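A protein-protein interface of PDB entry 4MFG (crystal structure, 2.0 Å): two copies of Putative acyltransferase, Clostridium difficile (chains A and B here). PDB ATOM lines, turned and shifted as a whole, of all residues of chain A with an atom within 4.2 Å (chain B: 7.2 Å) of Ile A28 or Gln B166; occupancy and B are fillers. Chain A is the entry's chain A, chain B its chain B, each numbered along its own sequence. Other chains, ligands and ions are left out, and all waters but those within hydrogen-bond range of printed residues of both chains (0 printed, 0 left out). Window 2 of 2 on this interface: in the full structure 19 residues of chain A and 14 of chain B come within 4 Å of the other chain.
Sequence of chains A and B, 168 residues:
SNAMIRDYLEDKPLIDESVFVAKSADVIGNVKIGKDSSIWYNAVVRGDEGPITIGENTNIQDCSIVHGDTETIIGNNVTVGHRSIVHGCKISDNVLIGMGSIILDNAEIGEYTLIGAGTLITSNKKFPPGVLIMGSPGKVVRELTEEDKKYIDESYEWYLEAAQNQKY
No position is printed for both chains.
Of the 9 pairs that touch across the chains among the printed residues, none has its exchanged pair printed and touching as well.
The guanidinium group of Arg A46 lies within salt-bridge range of the side-chain carboxylate of Asp B62.
OD2 of Asp A48 lies within hydrogen-bond range of NE2 of Gln B166 (3.1 Å).
N of Val A45 lies within hydrogen-bond range of O of Asp A26 (2.7 Å).
The backbone carbonyl oxygen (O) of Val A45 is in hydrogen-bond range of the backbone NH (N) of Ile A28.
The backbone carbonyl oxygen of Ile A28 sits at hydrogen-bond distance from the backbone NH of Gly A47, at 2.8 Å.
NH2 of Arg A46 lies within salt-bridge range of OD2 of Asp A48 (2.7 Å).
The backbone carbonyl oxygen of Ala B162 lies close to the side-chain amide oxygen of Gln B166 (2.6 Å).
Printed residues of chain B within 4 Å of Ile A28: Tyr B41 and Gln B166.
Of the printed residues of chain B, Arg A46 touches Trp B40, Tyr B41 and Asp B62.
Printed residues of chain B within 4 Å of Asp A48: Trp B40 (3.9 Å), Trp B158 (3.7 Å) and Gln B166 (3.1 Å).
Of the printed residues of chain A, Trp B40 touches Arg A46 (3.6 Å) and Asp A48 (3.9 Å).
Printed residues of chain A within 4 Å of Tyr B41: Asp A26, Ile A28 and Arg A46.
Printed residues of chain A within 4 Å of Trp B158: Asp A48 (3.7 Å).
Of the printed residues of chain A, Gln B166 touches Ile A28 (3.99 Å) and Asp A48 (3.1 Å).
The nearest printed residue of chain B that does not touch Ile A28 is Trp B40 (6.3 Å).
Hydrophobic or aromatic side chains of chain B within 4 Å of the printed part of chain A: Trp B40, Tyr B41 and Trp B158.
Hydrophobic or aromatic side chains of chain A that line the printed part of chain B: Ile A28.
Among the printed residues, 9 pairs touch across the chains.
Asp A26 touches Tyr B41.
CG2 of Ile A28 touches OH of Tyr B41 (3.6 Å).
Ile A28 touches Gln B166 (CG2 to NE2, 3.99 Å).
NH2 of Arg A46 touches CZ3 of Trp B40 (3.6 Å).
Arg A46 touches Tyr B41.
Trp B40 touches Asp A48.
Trp B158 touches Asp A48 (CH2 to OD1, 3.7 Å).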
ATOM      1  N   ASP A  26     -24.225  -0.979 -20.115  1.00  0.00           N
ATOM      2  CA  ASP A  26     -24.443  -1.966 -19.031  1.00  0.00           C
ATOM      3  C   ASP A  26     -23.463  -1.679 -17.902  1.00  0.00           C
ATOM      4  O   ASP A  26     -22.234  -1.702 -18.095  1.00  0.00           O
ATOM      5  CB  ASP A  26     -24.232  -3.382 -19.524  1.00  0.00           C
ATOM      6  CG  ASP A  26     -25.261  -3.805 -20.566  1.00  0.00           C
ATOM      7  OD1 ASP A  26     -26.469  -3.797 -20.222  1.00  0.00           O
ATOM      8  OD2 ASP A  26     -24.858  -4.185 -21.689  1.00  0.00           O
ATOM      9  N   VAL A  27     -24.004  -1.327 -16.738  1.00  0.00           N
ATOM     10  CA  VAL A  27     -23.192  -1.085 -15.558  1.00  0.00           C
ATOM     11  C   VAL A  27     -23.675  -2.199 -14.685  1.00  0.00           C
ATOM     12  O   VAL A  27     -24.831  -2.241 -14.334  1.00  0.00           O
ATOM     13  CB  VAL A  27     -23.413   0.301 -14.965  1.00  0.00           C
ATOM     14  CG1 VAL A  27     -22.453   0.534 -13.816  1.00  0.00           C
ATOM     15  CG2 VAL A  27     -23.166   1.352 -16.039  1.00  0.00           C
ATOM     16  N   ILE A  28     -22.792  -3.139 -14.396  1.00  0.00           N
ATOM     17  CA  ILE A  28     -23.198  -4.396 -13.800  1.00  0.00           C
ATOM     18  C   ILE A  28     -22.318  -4.800 -12.658  1.00  0.00           C
ATOM     19  O   ILE A  28     -21.113  -4.718 -12.776  1.00  0.00           O
ATOM     20  CB  ILE A  28     -23.036  -5.492 -14.888  1.00  0.00           C
ATOM     21  CG1 ILE A  28     -23.929  -5.177 -16.106  1.00  0.00           C
ATOM     22  CG2 ILE A  28     -23.383  -6.878 -14.368  1.00  0.00           C
ATOM     23  CD1 ILE A  28     -25.407  -5.279 -15.821  1.00  0.00           C
ATOM     24  N   GLY A  29     -22.910  -5.241 -11.559  1.00  0.00           N
ATOM     25  CA  GLY A  29     -22.123  -5.729 -10.439  1.00  0.00           C
ATOM     26  C   GLY A  29     -21.586  -4.672  -9.509  1.00  0.00           C
ATOM     27  O   GLY A  29     -22.213  -3.646  -9.310  1.00  0.00           O
ATOM     28  N   ASN A  30     -20.409  -4.940  -8.938  1.00  0.00           N
ATOM     29  CA  ASN A  30     -19.798  -4.067  -7.934  1.00  0.00           C
ATOM     30  C   ASN A  30     -19.036  -2.937  -8.595  1.00  0.00           C
ATOM     31  O   ASN A  30     -17.824  -3.039  -8.912  1.00  0.00           O
ATOM     32  CB  ASN A  30     -18.898  -4.872  -6.989  1.00  0.00           C
ATOM     33  CG  ASN A  30     -18.521  -4.092  -5.717  1.00  0.00           C
ATOM     34  OD1 ASN A  30     -18.364  -2.864  -5.730  1.00  0.00           O
ATOM     35  ND2 ASN A  30     -18.374  -4.816  -4.610  1.00  0.00           N
ATOM     36  N   VAL A  31     -19.759  -1.852  -8.800  1.00  0.00           N
ATOM     37  CA  VAL A  31     -19.241  -0.730  -9.493  1.00  0.00           C
ATOM     38  C   VAL A  31     -19.611   0.513  -8.770  1.00  0.00           C
ATOM     39  O   VAL A  31     -20.748   0.692  -8.369  1.00  0.00           O
ATOM     40  CB  VAL A  31     -19.867  -0.629 -10.884  1.00  0.00           C
ATOM     41  CG1 VAL A  31     -19.314   0.581 -11.619  1.00  0.00           C
ATOM     42  CG2 VAL A  31     -19.632  -1.909 -11.662  1.00  0.00           C
ATOM     43  N   VAL A  45     -19.497  -1.871 -18.100  1.00  0.00           N
ATOM     44  CA  VAL A  45     -18.712  -1.670 -16.913  1.00  0.00           C
ATOM     45  C   VAL A  45     -19.137  -2.789 -15.964  1.00  0.00           C
ATOM     46  O   VAL A  45     -20.138  -2.675 -15.294  1.00  0.00           O
ATOM     47  CB  VAL A  45     -18.963  -0.269 -16.332  1.00  0.00           C
ATOM     48  CG1 VAL A  45     -18.133  -0.056 -15.102  1.00  0.00           C
ATOM     49  CG2 VAL A  45     -18.644   0.796 -17.365  1.00  0.00           C
ATOM     50  N   ARG A  46     -18.345  -3.855 -15.906  1.00  0.00           N
ATOM     51  CA  ARG A  46     -18.748  -5.064 -15.185  1.00  0.00           C
ATOM     52  C   ARG A  46     -17.848  -5.404 -14.013  1.00  0.00           C
ATOM     53  O   ARG A  46     -16.740  -5.884 -14.200  1.00  0.00           O
ATOM     54  CB  ARG A  46     -18.789  -6.219 -16.190  1.00  0.00           C
ATOM     55  CG  ARG A  46     -19.236  -7.528 -15.607  1.00  0.00           C
ATOM     56  CD  ARG A  46     -19.790  -8.466 -16.650  1.00  0.00           C
ATOM     57  NE  ARG A  46     -18.861  -8.903 -17.692  1.00  0.00           N
ATOM     58  CZ  ARG A  46     -18.186 -10.051 -17.675  1.00  0.00           C
ATOM     59  NH1 ARG A  46     -17.412 -10.363 -18.699  1.00  0.00           N
ATOM     60  NH2 ARG A  46     -18.271 -10.887 -16.651  1.00  0.00           N
ATOM     61  N   GLY A  47     -18.338  -5.164 -12.803  1.00  0.00           N
ATOM     62  CA  GLY A  47     -17.561  -5.415 -11.587  1.00  0.00           C
ATOM     63  C   GLY A  47     -17.953  -6.692 -10.888  1.00  0.00           C
ATOM     64  O   GLY A  47     -18.109  -6.725  -9.685  1.00  0.00           O
ATOM     65  N   ASP A  48     -18.128  -7.750 -11.650  1.00  0.00           N
ATOM     66  CA  ASP A  48     -18.540  -9.033 -11.094  1.00  0.00           C
ATOM     67  C   ASP A  48     -17.364  -9.910 -10.705  1.00  0.00           C
ATOM     68  O   ASP A  48     -17.556 -10.991 -10.185  1.00  0.00           O
ATOM     69  CB  ASP A  48     -19.480  -9.775 -12.059  1.00  0.00           C
ATOM     70  CG  ASP A  48     -18.861 -10.049 -13.451  1.00  0.00           C
ATOM     71  OD1 ASP A  48     -17.668  -9.727 -13.709  1.00  0.00           O
ATOM     72  OD2 ASP A  48     -19.587 -10.614 -14.308  1.00  0.00           O
ATOM     73  N   PHE B  20     -26.705 -18.832 -20.868  1.00  0.00           N
ATOM     74  CA  PHE B  20     -26.992 -17.449 -20.456  1.00  0.00           C
ATOM     75  C   PHE B  20     -26.721 -16.508 -21.635  1.00  0.00           C
ATOM     76  O   PHE B  20     -25.660 -16.546 -22.237  1.00  0.00           O
ATOM     77  CB  PHE B  20     -26.160 -16.989 -19.243  1.00  0.00           C
ATOM     78  CG  PHE B  20     -26.154 -15.482 -19.035  1.00  0.00           C
ATOM     79  CD1 PHE B  20     -27.311 -14.804 -18.666  1.00  0.00           C
ATOM     80  CD2 PHE B  20     -24.987 -14.741 -19.203  1.00  0.00           C
ATOM     81  CE1 PHE B  20     -27.306 -13.427 -18.493  1.00  0.00           C
ATOM     82  CE2 PHE B  20     -24.987 -13.364 -19.020  1.00  0.00           C
ATOM     83  CZ  PHE B  20     -26.148 -12.710 -18.665  1.00  0.00           C
ATOM     84  N   ALA B  22     -26.958 -12.434 -22.259  1.00  0.00           N
ATOM     85  CA  ALA B  22     -27.259 -11.108 -21.707  1.00  0.00           C
ATOM     86  C   ALA B  22     -28.271 -10.402 -22.599  1.00  0.00           C
ATOM     87  O   ALA B  22     -28.254 -10.567 -23.810  1.00  0.00           O
ATOM     88  CB  ALA B  22     -26.009 -10.274 -21.582  1.00  0.00           C
ATOM     89  N   LYS B  23     -29.148  -9.626 -21.988  1.00  0.00           N
ATOM     90  CA  LYS B  23     -30.199  -8.918 -22.721  1.00  0.00           C
ATOM     91  C   LYS B  23     -29.606  -8.019 -23.787  1.00  0.00           C
ATOM     92  O   LYS B  23     -30.144  -7.925 -24.865  1.00  0.00           O
ATOM     93  CB  LYS B  23     -31.066  -8.117 -21.759  1.00  0.00           C
ATOM     94  CG  LYS B  23     -31.788  -9.008 -20.772  1.00  0.00           C
ATOM     95  CD  LYS B  23     -32.151  -8.284 -19.483  1.00  0.00           C
ATOM     96  CE  LYS B  23     -32.639  -9.258 -18.414  1.00  0.00           C
ATOM     97  NZ  LYS B  23     -33.873  -9.987 -18.813  1.00  0.00           N
ATOM     98  N   TRP B  40     -22.144 -12.778 -23.398  1.00  0.00           N
ATOM     99  CA  TRP B  40     -22.078 -11.609 -22.496  1.00  0.00           C
ATOM    100  C   TRP B  40     -22.523 -10.271 -23.064  1.00  0.00           C
ATOM    101  O   TRP B  40     -22.941 -10.184 -24.213  1.00  0.00           O
ATOM    102  CB  TRP B  40     -20.703 -11.554 -21.838  1.00  0.00           C
ATOM    103  CG  TRP B  40     -20.606 -12.700 -20.959  1.00  0.00           C
ATOM    104  CD1 TRP B  40     -20.305 -13.979 -21.311  1.00  0.00           C
ATOM    105  CD2 TRP B  40     -20.927 -12.720 -19.590  1.00  0.00           C
ATOM    106  NE1 TRP B  40     -20.392 -14.803 -20.218  1.00  0.00           N
ATOM    107  CE2 TRP B  40     -20.767 -14.046 -19.142  1.00  0.00           C
ATOM    108  CE3 TRP B  40     -21.341 -11.744 -18.682  1.00  0.00           C
ATOM    109  CZ2 TRP B  40     -21.002 -14.415 -17.827  1.00  0.00           C
ATOM    110  CZ3 TRP B  40     -21.566 -12.113 -17.371  1.00  0.00           C
ATOM    111  CH2 TRP B  40     -21.393 -13.438 -16.956  1.00  0.00           C
ATOM    112  N   TYR B  41     -22.484  -9.250 -22.207  1.00  0.00           N
ATOM    113  CA  TYR B  41     -23.029  -7.936 -22.546  1.00  0.00           C
ATOM    114  C   TYR B  41     -22.540  -7.366 -23.842  1.00  0.00           C
ATOM    115  O   TYR B  41     -21.356  -7.275 -24.100  1.00  0.00           O
ATOM    116  CB  TYR B  41     -22.821  -6.931 -21.399  1.00  0.00           C
ATOM    117  CG  TYR B  41     -23.429  -7.453 -20.125  1.00  0.00           C
ATOM    118  CD1 TYR B  41     -24.782  -7.245 -19.831  1.00  0.00           C
ATOM    119  CD2 TYR B  41     -22.698  -8.217 -19.270  1.00  0.00           C
ATOM    120  CE1 TYR B  41     -25.344  -7.748 -18.670  1.00  0.00           C
ATOM    121  CE2 TYR B  41     -23.262  -8.740 -18.117  1.00  0.00           C
ATOM    122  CZ  TYR B  41     -24.589  -8.489 -17.822  1.00  0.00           C
ATOM    123  OH  TYR B  41     -25.139  -9.009 -16.660  1.00  0.00           O
ATOM    124  N   ASP B  62     -18.012  -9.845 -23.307  1.00  0.00           N
ATOM    125  CA  ASP B  62     -18.625  -8.558 -23.633  1.00  0.00           C
ATOM    126  C   ASP B  62     -18.115  -7.939 -24.914  1.00  0.00           C
ATOM    127  O   ASP B  62     -16.932  -7.866 -25.160  1.00  0.00           O
ATOM    128  CB  ASP B  62     -18.426  -7.577 -22.486  1.00  0.00           C
ATOM    129  CG  ASP B  62     -18.463  -8.255 -21.150  1.00  0.00           C
ATOM    130  OD1 ASP B  62     -17.452  -8.874 -20.782  1.00  0.00           O
ATOM    131  OD2 ASP B  62     -19.473  -8.150 -20.463  1.00  0.00           O
ATOM    132  N   TRP B 158     -14.774 -20.369 -14.259  1.00  0.00           N
ATOM    133  CA  TRP B 158     -15.214 -19.146 -13.617  1.00  0.00           C
ATOM    134  C   TRP B 158     -16.460 -18.671 -14.299  1.00  0.00           C
ATOM    135  O   TRP B 158     -17.430 -18.298 -13.644  1.00  0.00           O
ATOM    136  CB  TRP B 158     -14.155 -18.052 -13.725  1.00  0.00           C
ATOM    137  CG  TRP B 158     -14.522 -16.844 -12.966  1.00  0.00           C
ATOM    138  CD1 TRP B 158     -14.266 -16.598 -11.653  1.00  0.00           C
ATOM    139  CD2 TRP B 158     -15.242 -15.720 -13.452  1.00  0.00           C
ATOM    140  NE1 TRP B 158     -14.764 -15.373 -11.297  1.00  0.00           N
ATOM    141  CE2 TRP B 158     -15.374 -14.815 -12.382  1.00  0.00           C
ATOM    142  CE3 TRP B 158     -15.777 -15.377 -14.702  1.00  0.00           C
ATOM    143  CZ2 TRP B 158     -16.030 -13.590 -12.512  1.00  0.00           C
ATOM    144  CZ3 TRP B 158     -16.433 -14.158 -14.833  1.00  0.00           C
ATOM    145  CH2 TRP B 158     -16.556 -13.282 -13.740  1.00  0.00           C
ATOM    146  N   GLU B 161     -19.713 -20.386 -13.485  1.00  0.00           N
ATOM    147  CA  GLU B 161     -20.198 -19.852 -12.209  1.00  0.00           C
ATOM    148  C   GLU B 161     -20.819 -18.453 -12.359  1.00  0.00           C
ATOM    149  O   GLU B 161     -21.971 -18.247 -12.020  1.00  0.00           O
ATOM    150  CB  GLU B 161     -19.039 -19.876 -11.175  1.00  0.00           C
ATOM    151  CG  GLU B 161     -19.230 -19.044  -9.918  1.00  0.00           C
ATOM    152  CD  GLU B 161     -20.364 -19.526  -9.052  1.00  0.00           C
ATOM    153  OE1 GLU B 161     -21.325 -18.743  -8.853  1.00  0.00           O
ATOM    154  OE2 GLU B 161     -20.315 -20.690  -8.592  1.00  0.00           O
ATOM    155  N   ALA B 162     -20.068 -17.495 -12.879  1.00  0.00           N
ATOM    156  CA  ALA B 162     -20.610 -16.152 -13.013  1.00  0.00           C
ATOM    157  C   ALA B 162     -21.885 -16.154 -13.833  1.00  0.00           C
ATOM    158  O   ALA B 162     -22.765 -15.347 -13.594  1.00  0.00           O
ATOM    159  CB  ALA B 162     -19.598 -15.220 -13.634  1.00  0.00           C
ATOM    160  N   ALA B 163     -21.981 -17.071 -14.794  1.00  0.00           N
ATOM    161  CA  ALA B 163     -23.168 -17.179 -15.642  1.00  0.00           C
ATOM    162  C   ALA B 163     -24.437 -17.500 -14.831  1.00  0.00           C
ATOM    163  O   ALA B 163     -25.512 -17.006 -15.139  1.00  0.00           O
ATOM    164  CB  ALA B 163     -22.951 -18.215 -16.739  1.00  0.00           C
ATOM    165  N   GLN B 164     -24.316 -18.320 -13.799  1.00  0.00           N
ATOM    166  CA  GLN B 164     -25.469 -18.625 -12.964  1.00  0.00           C
ATOM    167  C   GLN B 164     -25.912 -17.367 -12.227  1.00  0.00           C
ATOM    168  O   GLN B 164     -27.086 -16.972 -12.300  1.00  0.00           O
ATOM    169  CB  GLN B 164     -25.134 -19.713 -11.956  1.00  0.00           C
ATOM    170  CG  GLN B 164     -24.714 -21.033 -12.581  1.00  0.00           C
ATOM    171  CD  GLN B 164     -25.798 -21.681 -13.423  1.00  0.00           C
ATOM    172  OE1 GLN B 164     -25.493 -22.375 -14.393  1.00  0.00           O
ATOM    173  NE2 GLN B 164     -27.066 -21.465 -13.061  1.00  0.00           N
ATOM    174  N   ASN B 165     -24.965 -16.730 -11.536  1.00  0.00           N
ATOM    175  CA  ASN B 165     -25.267 -15.530 -10.761  1.00  0.00           C
ATOM    176  C   ASN B 165     -26.023 -14.444 -11.555  1.00  0.00           C
ATOM    177  O   ASN B 165     -26.939 -13.814 -11.027  1.00  0.00           O
ATOM    178  CB  ASN B 165     -23.997 -14.949 -10.149  1.00  0.00           C
ATOM    179  CG  ASN B 165     -23.331 -15.889  -9.150  1.00  0.00           C
ATOM    180  OD1 ASN B 165     -23.934 -16.834  -8.646  1.00  0.00           O
ATOM    181  ND2 ASN B 165     -22.070 -15.617  -8.855  1.00  0.00           N
ATOM    182  N   GLN B 166     -25.655 -14.245 -12.821  1.00  0.00           N
ATOM    183  CA  GLN B 166     -26.305 -13.235 -13.668  1.00  0.00           C
ATOM    184  C   GLN B 166     -27.753 -13.543 -14.032  1.00  0.00           C
ATOM    185  O   GLN B 166     -28.310 -12.885 -14.909  1.00  0.00           O
ATOM    186  CB  GLN B 166     -25.482 -12.918 -14.927  1.00  0.00           C
ATOM    187  CG  GLN B 166     -24.591 -11.675 -14.812  1.00  0.00           C
ATOM    188  CD  GLN B 166     -23.399 -11.810 -13.860  1.00  0.00           C
ATOM    189  OE1 GLN B 166     -23.187 -12.847 -13.237  1.00  0.00           O
ATOM    190  NE2 GLN B 166     -22.605 -10.749 -13.761  1.00  0.00           N
ATOM    191  N   LYS B 167     -28.345 -14.552 -13.382  1.00  0.00           N
ATOM    192  CA  LYS B 167     -29.801 -14.832 -13.530  1.00  0.00           C
ATOM    193  C   LYS B 167     -30.428 -15.716 -12.416  1.00  0.00           C
ATOM    194  O   LYS B 167     -31.602 -16.112 -12.504  1.00  0.00           O
ATOM    195  CB  LYS B 167     -30.182 -15.285 -14.959  1.00  0.00           C
ATOM    196  CG  LYS B 167     -29.177 -16.170 -15.690  1.00  0.00           C
ATOM    197  CD  LYS B 167     -29.122 -17.597 -15.189  1.00  0.00           C
ATOM    198  CE  LYS B 167     -28.349 -18.445 -16.185  1.00  0.00           C
ATOM    199  NZ  LYS B 167     -28.153 -19.851 -15.751  1.00  0.00           N
ATOM    200  N   TYR B 168     -29.646 -15.987 -11.366  1.00  0.00           N
ATOM    201  CA  TYR B 168     -30.110 -16.731 -10.174  1.00  0.00           C
ATOM    202  C   TYR B 168     -29.793 -15.993  -8.865  1.00  0.00           C
ATOM    203  O   TYR B 168     -30.585 -15.180  -8.375  1.00  0.00           O
ATOM    204  CB  TYR B 168     -29.510 -18.145 -10.105  1.00  0.00           C
ATOM    205  CG  TYR B 168     -30.463 -19.262 -10.463  1.00  0.00           C
ATOM    206  CD1 TYR B 168     -31.547 -19.549  -9.645  1.00  0.00           C
ATOM    207  CD2 TYR B 168     -30.244 -20.077 -11.569  1.00  0.00           C
ATOM    208  CE1 TYR B 168     -32.411 -20.579  -9.938  1.00  0.00           C
ATOM    209  CE2 TYR B 168     -31.109 -21.118 -11.867  1.00  0.00           C
ATOM    210  CZ  TYR B 168     -32.188 -21.362 -11.044  1.00  0.00           C
ATOM    211  OH  TYR B 168     -33.055 -22.391 -11.323  1.00  0.00           O
ATOM    212  OXT TYR B 168     -28.745 -16.209  -8.248  1.00  0.00           O
